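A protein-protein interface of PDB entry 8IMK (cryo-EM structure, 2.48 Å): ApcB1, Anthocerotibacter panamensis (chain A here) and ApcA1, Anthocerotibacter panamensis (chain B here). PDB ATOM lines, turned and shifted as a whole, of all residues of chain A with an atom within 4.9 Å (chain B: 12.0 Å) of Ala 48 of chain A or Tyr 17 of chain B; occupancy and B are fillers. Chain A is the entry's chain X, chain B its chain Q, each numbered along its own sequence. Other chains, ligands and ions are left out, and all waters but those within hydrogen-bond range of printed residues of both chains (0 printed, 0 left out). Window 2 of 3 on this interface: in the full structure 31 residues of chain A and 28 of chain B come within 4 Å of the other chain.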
ATOM      1  N   ILE A  44      -2.565  -9.618  18.635  1.00  0.00           N
ATOM      2  CA  ILE A  44      -1.956 -10.513  19.614  1.00  0.00           C
ATOM      3  C   ILE A  44      -3.001 -11.013  20.600  1.00  0.00           C
ATOM      4  O   ILE A  44      -3.033 -12.198  20.948  1.00  0.00           O
ATOM      5  CB  ILE A  44      -0.796  -9.812  20.338  1.00  0.00           C
ATOM      6  CG1 ILE A  44       0.389  -9.638  19.398  1.00  0.00           C
ATOM      7  CG2 ILE A  44      -0.393 -10.592  21.573  1.00  0.00           C
ATOM      8  CD1 ILE A  44       1.535  -8.908  20.027  1.00  0.00           C
ATOM      9  N   SER A  45      -3.872 -10.119  21.066  1.00  0.00           N
ATOM     10  CA  SER A  45      -4.887 -10.499  22.038  1.00  0.00           C
ATOM     11  C   SER A  45      -5.850 -11.530  21.468  1.00  0.00           C
ATOM     12  O   SER A  45      -6.246 -12.472  22.159  1.00  0.00           O
ATOM     13  CB  SER A  45      -5.644  -9.258  22.497  1.00  0.00           C
ATOM     14  OG  SER A  45      -6.810  -9.607  23.213  1.00  0.00           O
ATOM     15  N   ALA A  46      -6.255 -11.351  20.211  1.00  0.00           N
ATOM     16  CA  ALA A  46      -7.231 -12.249  19.610  1.00  0.00           C
ATOM     17  C   ALA A  46      -6.644 -13.635  19.387  1.00  0.00           C
ATOM     18  O   ALA A  46      -7.352 -14.641  19.491  1.00  0.00           O
ATOM     19  CB  ALA A  46      -7.729 -11.659  18.295  1.00  0.00           C
ATOM     20  N   ASN A  47      -5.351 -13.704  19.094  1.00  0.00           N
ATOM     21  CA  ASN A  47      -4.669 -14.939  18.751  1.00  0.00           C
ATOM     22  C   ASN A  47      -3.752 -15.427  19.859  1.00  0.00           C
ATOM     23  O   ASN A  47      -2.830 -16.200  19.589  1.00  0.00           O
ATOM     24  CB  ASN A  47      -3.875 -14.742  17.463  1.00  0.00           C
ATOM     25  CG  ASN A  47      -4.750 -14.344  16.309  1.00  0.00           C
ATOM     26  OD1 ASN A  47      -4.705 -13.209  15.845  1.00  0.00           O
ATOM     27  ND2 ASN A  47      -5.558 -15.280  15.834  1.00  0.00           N
ATOM     28  N   ALA A  48      -3.999 -15.012  21.102  1.00  0.00           N
ATOM     29  CA  ALA A  48      -3.082 -15.332  22.189  1.00  0.00           C
ATOM     30  C   ALA A  48      -2.966 -16.835  22.410  1.00  0.00           C
ATOM     31  O   ALA A  48      -1.870 -17.346  22.655  1.00  0.00           O
ATOM     32  CB  ALA A  48      -3.527 -14.631  23.469  1.00  0.00           C
ATOM     33  N   ALA A  49      -4.082 -17.562  22.329  1.00  0.00           N
ATOM     34  CA  ALA A  49      -4.036 -19.010  22.507  1.00  0.00           C
ATOM     35  C   ALA A  49      -3.186 -19.677  21.435  1.00  0.00           C
ATOM     36  O   ALA A  49      -2.364 -20.551  21.732  1.00  0.00           O
ATOM     37  CB  ALA A  49      -5.450 -19.579  22.497  1.00  0.00           C
ATOM     38  N   SER A  50      -3.368 -19.275  20.179  1.00  0.00           N
ATOM     39  CA  SER A  50      -2.560 -19.822  19.098  1.00  0.00           C
ATOM     40  C   SER A  50      -1.088 -19.478  19.278  1.00  0.00           C
ATOM     41  O   SER A  50      -0.213 -20.313  19.026  1.00  0.00           O
ATOM     42  CB  SER A  50      -3.075 -19.307  17.757  1.00  0.00           C
ATOM     43  OG  SER A  50      -2.465 -19.991  16.681  1.00  0.00           O
ATOM     44  N   ILE A  51      -0.795 -18.253  19.716  1.00  0.00           N
ATOM     45  CA  ILE A  51       0.589 -17.847  19.924  1.00  0.00           C
ATOM     46  C   ILE A  51       1.239 -18.699  21.004  1.00  0.00           C
ATOM     47  O   ILE A  51       2.355 -19.197  20.830  1.00  0.00           O
ATOM     48  CB  ILE A  51       0.660 -16.346  20.267  1.00  0.00           C
ATOM     49  CG1 ILE A  51       0.170 -15.502  19.095  1.00  0.00           C
ATOM     50  CG2 ILE A  51       2.071 -15.948  20.631  1.00  0.00           C
ATOM     51  CD1 ILE A  51      -0.221 -14.094  19.480  1.00  0.00           C
ATOM     52  N   LEU A  52       0.555 -18.880  22.137  1.00  0.00           N
ATOM     53  CA  LEU A  52       1.087 -19.737  23.190  1.00  0.00           C
ATOM     54  C   LEU A  52       1.285 -21.163  22.713  1.00  0.00           C
ATOM     55  O   LEU A  52       2.310 -21.779  23.009  1.00  0.00           O
ATOM     56  CB  LEU A  52       0.184 -19.710  24.423  1.00  0.00           C
ATOM     57  CG  LEU A  52       0.367 -18.573  25.423  1.00  0.00           C
ATOM     58  CD1 LEU A  52       1.734 -18.720  26.010  1.00  0.00           C
ATOM     59  CD2 LEU A  52       0.266 -17.216  24.788  1.00  0.00           C
ATOM     60  N   GLU A  87       2.490 -16.981  28.861  1.00  0.00           N
ATOM     61  CA  GLU A  87       1.301 -16.134  28.819  1.00  0.00           C
ATOM     62  C   GLU A  87       1.556 -14.774  29.461  1.00  0.00           C
ATOM     63  O   GLU A  87       1.138 -13.741  28.929  1.00  0.00           O
ATOM     64  CB  GLU A  87       0.145 -16.847  29.518  1.00  0.00           C
ATOM     65  CG  GLU A  87      -1.174 -16.099  29.524  1.00  0.00           C
ATOM     66  CD  GLU A  87      -1.769 -15.912  28.150  1.00  0.00           C
ATOM     67  OE1 GLU A  87      -1.476 -16.732  27.262  1.00  0.00           O
ATOM     68  OE2 GLU A  87      -2.528 -14.939  27.955  1.00  0.00           O
ATOM     69  N   LEU A  90       3.695 -12.646  27.041  1.00  0.00           N
ATOM     70  CA  LEU A  90       2.924 -12.113  25.924  1.00  0.00           C
ATOM     71  C   LEU A  90       1.976 -11.003  26.366  1.00  0.00           C
ATOM     72  O   LEU A  90       1.862  -9.972  25.694  1.00  0.00           O
ATOM     73  CB  LEU A  90       2.151 -13.237  25.244  1.00  0.00           C
ATOM     74  CG  LEU A  90       1.419 -12.855  23.963  1.00  0.00           C
ATOM     75  CD1 LEU A  90       2.385 -12.675  22.820  1.00  0.00           C
ATOM     76  CD2 LEU A  90       0.369 -13.875  23.625  1.00  0.00           C
ATOM     77  N   ARG A  91       1.276 -11.201  27.484  1.00  0.00           N
ATOM     78  CA  ARG A  91       0.323 -10.201  27.946  1.00  0.00           C
ATOM     79  C   ARG A  91       1.023  -8.887  28.268  1.00  0.00           C
ATOM     80  O   ARG A  91       0.571  -7.808  27.861  1.00  0.00           O
ATOM     81  CB  ARG A  91      -0.433 -10.738  29.159  1.00  0.00           C
ATOM     82  CG  ARG A  91      -1.332  -9.735  29.828  1.00  0.00           C
ATOM     83  CD  ARG A  91      -2.395 -10.398  30.675  1.00  0.00           C
ATOM     84  NE  ARG A  91      -1.850 -11.254  31.723  1.00  0.00           N
ATOM     85  CZ  ARG A  91      -1.631 -10.866  32.973  1.00  0.00           C
ATOM     86  NH1 ARG A  91      -1.903  -9.626  33.344  1.00  0.00           N
ATOM     87  NH2 ARG A  91      -1.144 -11.723  33.854  1.00  0.00           N
ATOM     88  N   THR A  94       2.164  -7.069  25.211  1.00  0.00           N
ATOM     89  CA  THR A  94       1.066  -6.314  24.616  1.00  0.00           C
ATOM     90  C   THR A  94       0.813  -5.013  25.370  1.00  0.00           C
ATOM     91  O   THR A  94       0.570  -3.965  24.756  1.00  0.00           O
ATOM     92  CB  THR A  94      -0.193  -7.176  24.582  1.00  0.00           C
ATOM     93  OG1 THR A  94       0.112  -8.433  23.976  1.00  0.00           O
ATOM     94  CG2 THR A  94      -1.268  -6.510  23.787  1.00  0.00           C
ATOM     95  N   TYR A  95       0.859  -5.063  26.703  1.00  0.00           N
ATOM     96  CA  TYR A  95       0.742  -3.837  27.489  1.00  0.00           C
ATOM     97  C   TYR A  95       1.810  -2.830  27.094  1.00  0.00           C
ATOM     98  O   TYR A  95       1.508  -1.664  26.834  1.00  0.00           O
ATOM     99  CB  TYR A  95       0.865  -4.128  28.981  1.00  0.00           C
ATOM    100  CG  TYR A  95      -0.263  -4.902  29.596  1.00  0.00           C
ATOM    101  CD1 TYR A  95      -1.503  -4.966  28.991  1.00  0.00           C
ATOM    102  CD2 TYR A  95      -0.085  -5.564  30.800  1.00  0.00           C
ATOM    103  CE1 TYR A  95      -2.525  -5.671  29.564  1.00  0.00           C
ATOM    104  CE2 TYR A  95      -1.101  -6.266  31.378  1.00  0.00           C
ATOM    105  CZ  TYR A  95      -2.317  -6.320  30.755  1.00  0.00           C
ATOM    106  OH  TYR A  95      -3.338  -7.025  31.336  1.00  0.00           O
ATOM    107  N   ILE B   4      -4.092   5.793  28.391  1.00  0.00           N
ATOM    108  CA  ILE B   4      -3.473   4.498  28.148  1.00  0.00           C
ATOM    109  C   ILE B   4      -3.029   3.858  29.454  1.00  0.00           C
ATOM    110  O   ILE B   4      -3.242   2.663  29.675  1.00  0.00           O
ATOM    111  CB  ILE B   4      -2.298   4.655  27.168  1.00  0.00           C
ATOM    112  CG1 ILE B   4      -2.816   4.840  25.746  1.00  0.00           C
ATOM    113  CG2 ILE B   4      -1.368   3.464  27.250  1.00  0.00           C
ATOM    114  CD1 ILE B   4      -1.733   5.082  24.747  1.00  0.00           C
ATOM    115  N   THR B   5      -2.395   4.634  30.332  1.00  0.00           N
ATOM    116  CA  THR B   5      -1.937   4.092  31.606  1.00  0.00           C
ATOM    117  C   THR B   5      -3.102   3.616  32.458  1.00  0.00           C
ATOM    118  O   THR B   5      -3.027   2.556  33.086  1.00  0.00           O
ATOM    119  CB  THR B   5      -1.121   5.140  32.358  1.00  0.00           C
ATOM    120  OG1 THR B   5       0.018   5.510  31.579  1.00  0.00           O
ATOM    121  CG2 THR B   5      -0.673   4.607  33.703  1.00  0.00           C
ATOM    122  N   LYS B   6      -4.189   4.382  32.491  1.00  0.00           N
ATOM    123  CA  LYS B   6      -5.350   3.975  33.269  1.00  0.00           C
ATOM    124  C   LYS B   6      -5.943   2.681  32.724  1.00  0.00           C
ATOM    125  O   LYS B   6      -6.213   1.744  33.487  1.00  0.00           O
ATOM    126  CB  LYS B   6      -6.367   5.120  33.281  1.00  0.00           C
ATOM    127  CG  LYS B   6      -7.568   4.951  34.189  1.00  0.00           C
ATOM    128  CD  LYS B   6      -8.746   4.306  33.488  1.00  0.00           C
ATOM    129  CE  LYS B   6      -9.944   4.230  34.417  1.00  0.00           C
ATOM    130  NZ  LYS B   6     -11.103   3.568  33.767  1.00  0.00           N
ATOM    131  N   ALA B   7      -6.102   2.588  31.399  1.00  0.00           N
ATOM    132  CA  ALA B   7      -6.648   1.370  30.806  1.00  0.00           C
ATOM    133  C   ALA B   7      -5.749   0.166  31.061  1.00  0.00           C
ATOM    134  O   ALA B   7      -6.234  -0.920  31.406  1.00  0.00           O
ATOM    135  CB  ALA B   7      -6.857   1.569  29.306  1.00  0.00           C
ATOM    136  N   ILE B   8      -4.438   0.331  30.893  1.00  0.00           N
ATOM    137  CA  ILE B   8      -3.529  -0.789  31.094  1.00  0.00           C
ATOM    138  C   ILE B   8      -3.514  -1.207  32.555  1.00  0.00           C
ATOM    139  O   ILE B   8      -3.425  -2.396  32.865  1.00  0.00           O
ATOM    140  CB  ILE B   8      -2.117  -0.447  30.593  1.00  0.00           C
ATOM    141  CG1 ILE B   8      -2.101  -0.361  29.072  1.00  0.00           C
ATOM    142  CG2 ILE B   8      -1.127  -1.492  31.055  1.00  0.00           C
ATOM    143  CD1 ILE B   8      -0.791   0.086  28.517  1.00  0.00           C
ATOM    144  N   LEU B   9      -3.595  -0.250  33.477  1.00  0.00           N
ATOM    145  CA  LEU B   9      -3.617  -0.602  34.889  1.00  0.00           C
ATOM    146  C   LEU B   9      -4.886  -1.363  35.243  1.00  0.00           C
ATOM    147  O   LEU B   9      -4.844  -2.318  36.022  1.00  0.00           O
ATOM    148  CB  LEU B   9      -3.471   0.649  35.748  1.00  0.00           C
ATOM    149  CG  LEU B   9      -3.412   0.409  37.255  1.00  0.00           C
ATOM    150  CD1 LEU B   9      -2.195  -0.420  37.608  1.00  0.00           C
ATOM    151  CD2 LEU B   9      -3.390   1.720  38.005  1.00  0.00           C
ATOM    152  N   ASN B  10      -6.023  -0.967  34.669  1.00  0.00           N
ATOM    153  CA  ASN B  10      -7.241  -1.740  34.897  1.00  0.00           C
ATOM    154  C   ASN B  10      -7.119  -3.153  34.348  1.00  0.00           C
ATOM    155  O   ASN B  10      -7.539  -4.110  35.001  1.00  0.00           O
ATOM    156  CB  ASN B  10      -8.460  -1.048  34.295  1.00  0.00           C
ATOM    157  CG  ASN B  10      -8.755   0.276  34.945  1.00  0.00           C
ATOM    158  OD1 ASN B  10      -8.664   1.323  34.315  1.00  0.00           O
ATOM    159  ND2 ASN B  10      -9.103   0.240  36.223  1.00  0.00           N
ATOM    160  N   ALA B  11      -6.566  -3.305  33.143  1.00  0.00           N
ATOM    161  CA  ALA B  11      -6.399  -4.648  32.597  1.00  0.00           C
ATOM    162  C   ALA B  11      -5.460  -5.479  33.457  1.00  0.00           C
ATOM    163  O   ALA B  11      -5.741  -6.642  33.753  1.00  0.00           O
ATOM    164  CB  ALA B  11      -5.888  -4.578  31.162  1.00  0.00           C
ATOM    165  N   ASP B  12      -4.349  -4.886  33.877  1.00  0.00           N
ATOM    166  CA  ASP B  12      -3.350  -5.601  34.657  1.00  0.00           C
ATOM    167  C   ASP B  12      -3.895  -6.020  36.014  1.00  0.00           C
ATOM    168  O   ASP B  12      -3.609  -7.123  36.491  1.00  0.00           O
ATOM    169  CB  ASP B  12      -2.119  -4.720  34.811  1.00  0.00           C
ATOM    170  CG  ASP B  12      -0.926  -5.473  35.310  1.00  0.00           C
ATOM    171  OD1 ASP B  12      -0.840  -6.687  35.058  1.00  0.00           O
ATOM    172  OD2 ASP B  12      -0.063  -4.848  35.948  1.00  0.00           O
ATOM    173  N   ALA B  13      -4.671  -5.147  36.658  1.00  0.00           N
ATOM    174  CA  ALA B  13      -5.250  -5.482  37.953  1.00  0.00           C
ATOM    175  C   ALA B  13      -6.236  -6.634  37.834  1.00  0.00           C
ATOM    176  O   ALA B  13      -6.425  -7.398  38.785  1.00  0.00           O
ATOM    177  CB  ALA B  13      -5.921  -4.250  38.560  1.00  0.00           C
ATOM    178  N   GLU B  14      -6.873  -6.780  36.677  1.00  0.00           N
ATOM    179  CA  GLU B  14      -7.758  -7.906  36.420  1.00  0.00           C
ATOM    180  C   GLU B  14      -7.074  -9.050  35.688  1.00  0.00           C
ATOM    181  O   GLU B  14      -7.736 -10.042  35.378  1.00  0.00           O
ATOM    182  CB  GLU B  14      -8.977  -7.452  35.621  1.00  0.00           C
ATOM    183  CG  GLU B  14      -9.582  -6.161  36.106  1.00  0.00           C
ATOM    184  CD  GLU B  14     -11.049  -6.045  35.763  1.00  0.00           C
ATOM    185  OE1 GLU B  14     -11.463  -4.976  35.269  1.00  0.00           O
ATOM    186  OE2 GLU B  14     -11.789  -7.024  35.990  1.00  0.00           O
ATOM    187  N   ALA B  15      -5.778  -8.922  35.391  1.00  0.00           N
ATOM    188  CA  ALA B  15      -4.976  -9.984  34.774  1.00  0.00           C
ATOM    189  C   ALA B  15      -5.547 -10.431  33.434  1.00  0.00           C
ATOM    190  O   ALA B  15      -5.782 -11.615  33.202  1.00  0.00           O
ATOM    191  CB  ALA B  15      -4.825 -11.177  35.714  1.00  0.00           C
ATOM    192  N   ARG B  16      -5.763  -9.481  32.536  1.00  0.00           N
ATOM    193  CA  ARG B  16      -6.419  -9.758  31.273  1.00  0.00           C
ATOM    194  C   ARG B  16      -5.889  -8.812  30.212  1.00  0.00           C
ATOM    195  O   ARG B  16      -5.285  -7.782  30.510  1.00  0.00           O
ATOM    196  CB  ARG B  16      -7.934  -9.611  31.392  1.00  0.00           C
ATOM    197  CG  ARG B  16      -8.348  -8.280  31.941  1.00  0.00           C
ATOM    198  CD  ARG B  16      -9.841  -8.146  31.994  1.00  0.00           C
ATOM    199  NE  ARG B  16     -10.233  -6.795  32.380  1.00  0.00           N
ATOM    200  CZ  ARG B  16     -10.070  -5.719  31.619  1.00  0.00           C
ATOM    201  NH1 ARG B  16      -9.531  -5.821  30.416  1.00  0.00           N
ATOM    202  NH2 ARG B  16     -10.453  -4.535  32.064  1.00  0.00           N
ATOM    203  N   TYR B  17      -6.121  -9.176  28.960  1.00  0.00           N
ATOM    204  CA  TYR B  17      -5.809  -8.287  27.857  1.00  0.00           C
ATOM    205  C   TYR B  17      -6.774  -7.109  27.843  1.00  0.00           C
ATOM    206  O   TYR B  17      -7.808  -7.113  28.513  1.00  0.00           O
ATOM    207  CB  TYR B  17      -5.874  -9.044  26.536  1.00  0.00           C
ATOM    208  CG  TYR B  17      -4.732 -10.004  26.349  1.00  0.00           C
ATOM    209  CD1 TYR B  17      -4.856 -11.332  26.709  1.00  0.00           C
ATOM    210  CD2 TYR B  17      -3.527  -9.579  25.833  1.00  0.00           C
ATOM    211  CE1 TYR B  17      -3.817 -12.204  26.557  1.00  0.00           C
ATOM    212  CE2 TYR B  17      -2.481 -10.450  25.667  1.00  0.00           C
ATOM    213  CZ  TYR B  17      -2.632 -11.760  26.030  1.00  0.00           C
ATOM    214  OH  TYR B  17      -1.590 -12.632  25.867  1.00  0.00           O
ATOM    215  N   LEU B  18      -6.419  -6.083  27.078  1.00  0.00           N
ATOM    216  CA  LEU B  18      -7.292  -4.925  26.959  1.00  0.00           C
ATOM    217  C   LEU B  18      -8.610  -5.331  26.316  1.00  0.00           C
ATOM    218  O   LEU B  18      -8.632  -6.009  25.285  1.00  0.00           O
ATOM    219  CB  LEU B  18      -6.618  -3.826  26.144  1.00  0.00           C
ATOM    220  CG  LEU B  18      -5.362  -3.167  26.718  1.00  0.00           C
ATOM    221  CD1 LEU B  18      -4.779  -2.209  25.702  1.00  0.00           C
ATOM    222  CD2 LEU B  18      -5.652  -2.442  28.015  1.00  0.00           C
ATOM    223  N   SER B  19      -9.705  -4.921  26.933  1.00  0.00           N
ATOM    224  CA  SER B  19     -11.037  -5.274  26.480  1.00  0.00           C
ATOM    225  C   SER B  19     -11.419  -4.425  25.277  1.00  0.00           C
ATOM    226  O   SER B  19     -10.743  -3.451  24.953  1.00  0.00           O
ATOM    227  CB  SER B  19     -12.028  -5.097  27.625  1.00  0.00           C
ATOM    228  OG  SER B  19     -11.783  -3.902  28.337  1.00  0.00           O
ATOM    229  N   PRO B  20     -12.489  -4.792  24.566  1.00  0.00           N
ATOM    230  CA  PRO B  20     -12.949  -3.925  23.469  1.00  0.00           C
ATOM    231  C   PRO B  20     -13.219  -2.495  23.903  1.00  0.00           C
ATOM    232  O   PRO B  20     -12.903  -1.559  23.160  1.00  0.00           O
ATOM    233  CB  PRO B  20     -14.227  -4.624  22.992  1.00  0.00           C
ATOM    234  CG  PRO B  20     -14.020  -6.043  23.327  1.00  0.00           C
ATOM    235  CD  PRO B  20     -13.189  -6.090  24.572  1.00  0.00           C
ATOM    236  N   GLY B  21     -13.784  -2.295  25.094  1.00  0.00           N
ATOM    237  CA  GLY B  21     -14.016  -0.944  25.578  1.00  0.00           C
ATOM    238  C   GLY B  21     -12.732  -0.193  25.874  1.00  0.00           C
ATOM    239  O   GLY B  21     -12.609   0.993  25.563  1.00  0.00           O
ATOM    240  N   GLU B  22     -11.758  -0.874  26.475  1.00  0.00           N
ATOM    241  CA  GLU B  22     -10.460  -0.257  26.719  1.00  0.00           C
ATOM    242  C   GLU B  22      -9.768   0.091  25.409  1.00  0.00           C
ATOM    243  O   GLU B  22      -9.152   1.158  25.283  1.00  0.00           O
ATOM    244  CB  GLU B  22      -9.593  -1.197  27.552  1.00  0.00           C
ATOM    245  CG  GLU B  22      -9.745  -1.025  29.048  1.00  0.00           C
ATOM    246  CD  GLU B  22      -9.364  -2.273  29.818  1.00  0.00           C
ATOM    247  OE1 GLU B  22      -9.534  -2.289  31.052  1.00  0.00           O
ATOM    248  OE2 GLU B  22      -8.905  -3.243  29.186  1.00  0.00           O
ATOM    249  N   ILE B  23      -9.867  -0.800  24.421  1.00  0.00           N
ATOM    250  CA  ILE B  23      -9.286  -0.540  23.109  1.00  0.00           C
ATOM    251  C   ILE B  23      -9.944   0.671  22.463  1.00  0.00           C
ATOM    252  O   ILE B  23      -9.269   1.509  21.861  1.00  0.00           O
ATOM    253  CB  ILE B  23      -9.394  -1.794  22.223  1.00  0.00           C
ATOM    254  CG1 ILE B  23      -8.477  -2.895  22.754  1.00  0.00           C
ATOM    255  CG2 ILE B  23      -9.062  -1.469  20.786  1.00  0.00           C
ATOM    256  CD1 ILE B  23      -7.026  -2.672  22.458  1.00  0.00           C
ATOM    257  N   ASP B  24     -11.269   0.785  22.578  1.00  0.00           N
ATOM    258  CA  ASP B  24     -11.967   1.942  22.021  1.00  0.00           C
ATOM    259  C   ASP B  24     -11.583   3.232  22.740  1.00  0.00           C
ATOM    260  O   ASP B  24     -11.467   4.289  22.112  1.00  0.00           O
ATOM    261  CB  ASP B  24     -13.475   1.722  22.085  1.00  0.00           C
ATOM    262  CG  ASP B  24     -14.010   1.027  20.855  1.00  0.00           C
ATOM    263  OD1 ASP B  24     -13.548   1.353  19.743  1.00  0.00           O
ATOM    264  OD2 ASP B  24     -14.892   0.153  21.000  1.00  0.00           O
ATOM    265  N   VAL B  25     -11.380   3.164  24.057  1.00  0.00           N
ATOM    266  CA  VAL B  25     -10.908   4.328  24.804  1.00  0.00           C
ATOM    267  C   VAL B  25      -9.549   4.777  24.290  1.00  0.00           C
ATOM    268  O   VAL B  25      -9.314   5.970  24.042  1.00  0.00           O
ATOM    269  CB  VAL B  25     -10.848   4.001  26.307  1.00  0.00           C
ATOM    270  CG1 VAL B  25     -10.003   5.022  27.047  1.00  0.00           C
ATOM    271  CG2 VAL B  25     -12.237   3.919  26.886  1.00  0.00           C
ATOM    272  N   VAL B  26      -8.633   3.825  24.119  1.00  0.00           N
ATOM    273  CA  VAL B  26      -7.291   4.155  23.660  1.00  0.00           C
ATOM    274  C   VAL B  26      -7.330   4.704  22.241  1.00  0.00           C
ATOM    275  O   VAL B  26      -6.609   5.652  21.908  1.00  0.00           O
ATOM    276  CB  VAL B  26      -6.376   2.926  23.774  1.00  0.00           C
ATOM    277  CG1 VAL B  26      -5.060   3.202  23.101  1.00  0.00           C
ATOM    278  CG2 VAL B  26      -6.165   2.560  25.224  1.00  0.00           C
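The side-chain carboxylate of Asp 12 of chain B lies within salt-bridge range of the guanidinium group of Arg 91 of chain A, 3.6 Å away.
The backbone carbonyl oxygen of Arg 16 of chain B sits close to the side-chain hydroxyl of Tyr 95 of chain A (2.2 Å).
The side-chain hydroxyl (OH) of Tyr 17 of chain B is in hydrogen-bond range of the side-chain carboxylate (OE2) of Glu 87 of chain A, at 3.2 Å.
N of Asp 12 of chain B sits at hydrogen-bond distance from OH of Tyr 95 of chain A, at 3.5 Å.
O of Ala 11 of chain B sits close to OH of Tyr 95 of chain A, 3.4 Å away.
O of Ala 11 of chain B sits at hydrogen-bond distance from N of Arg 16 of chain B, at 3.1 Å.
OE1 of Glu 22 of chain B is in salt-bridge range of NH2 of Arg 16 of chain B (2.6 Å).
NH2 of Arg 16 of chain B is in salt-bridge range of OE1 of Glu 14 of chain B, 3.4 Å away.
The backbone carbonyl oxygen (O) of Leu 90 of chain A lies within hydrogen-bond range of the side-chain hydroxyl (OG1) of Thr 94 of chain A, 2.9 Å away.
Of the 23 printed residues of chain B, 6 touch a printed residue of chain A.
Hydrophobic or aromatic side chains of chain B within 4 Å of the printed part of chain A: Ile 8, Ala 11 and Tyr 17.
Along chain B the printed residues that touch a printed residue of chain A span positions 8 to 17.
Among the printed residues, 13 pairs touch across the chains.
Among the printed residues, Asp or Glu carboxylates within 4 Å of a Lys or Arg side-chain nitrogen of the other chain: Arg 91 of chain A with Asp 12 of chain B (3.6 Å).
Among the printed residues, pairs that only touch across the chains: Ser 45 of chain A with Tyr 17 of chain B (3.5 Å), Ala 48 of chain A with Tyr 17 of chain B (3.7 Å), Leu 90 of chain A with Tyr 17 of chain B (3.2 Å), Arg 91 of chain A with Ala 15 of chain B (3.4 Å), Arg 91 of chain A with Arg 16 of chain B (3.9 Å), Arg 91 of chain A with Tyr 17 of chain B (3.6 Å), Thr 94 of chain A with Tyr 17 of chain B (3.7 Å) and Tyr 95 of chain A with Ile 8 of chain B (3.3 Å).
No residue of chain B comes within 4 Å of Ile 44 of chain A.
No residue of chain B comes within 4 Å of Ala 46 of chain A.
Of chain B, only Tyr 17 (3.7 Å) comes within 4 Å of Ala 48 of chain A.
No residue of chain B comes within 4 Å of Ser 50 of chain A.
No residue of chain B comes within 4 Å of Ile 51 of chain A.
Of chain B, only Tyr 17 (3.2 Å) comes within 4 Å of Leu 90 of chain A.
Arg 91 of chain A touches just these residues of chain B: Asp 12 (3.6 Å), Ala 15 (3.4 Å), Arg 16 (3.9 Å) and Tyr 17 (3.6 Å).
Thr 94 of chain A touches one residue of chain B.
Of the printed residues of chain B, Tyr 95 of chain A touches Ile 8, Ala 11, Asp 12 and Arg 16.
Printed residues of chain A within 4 Å of Asp 12 of chain B: Arg 91 (3.6 Å) and Tyr 95 (3.5 Å).
Ser 19 of chain B touches none of the printed residues of chain A.
Val 25 of chain B touches none of the printed residues of chain A.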
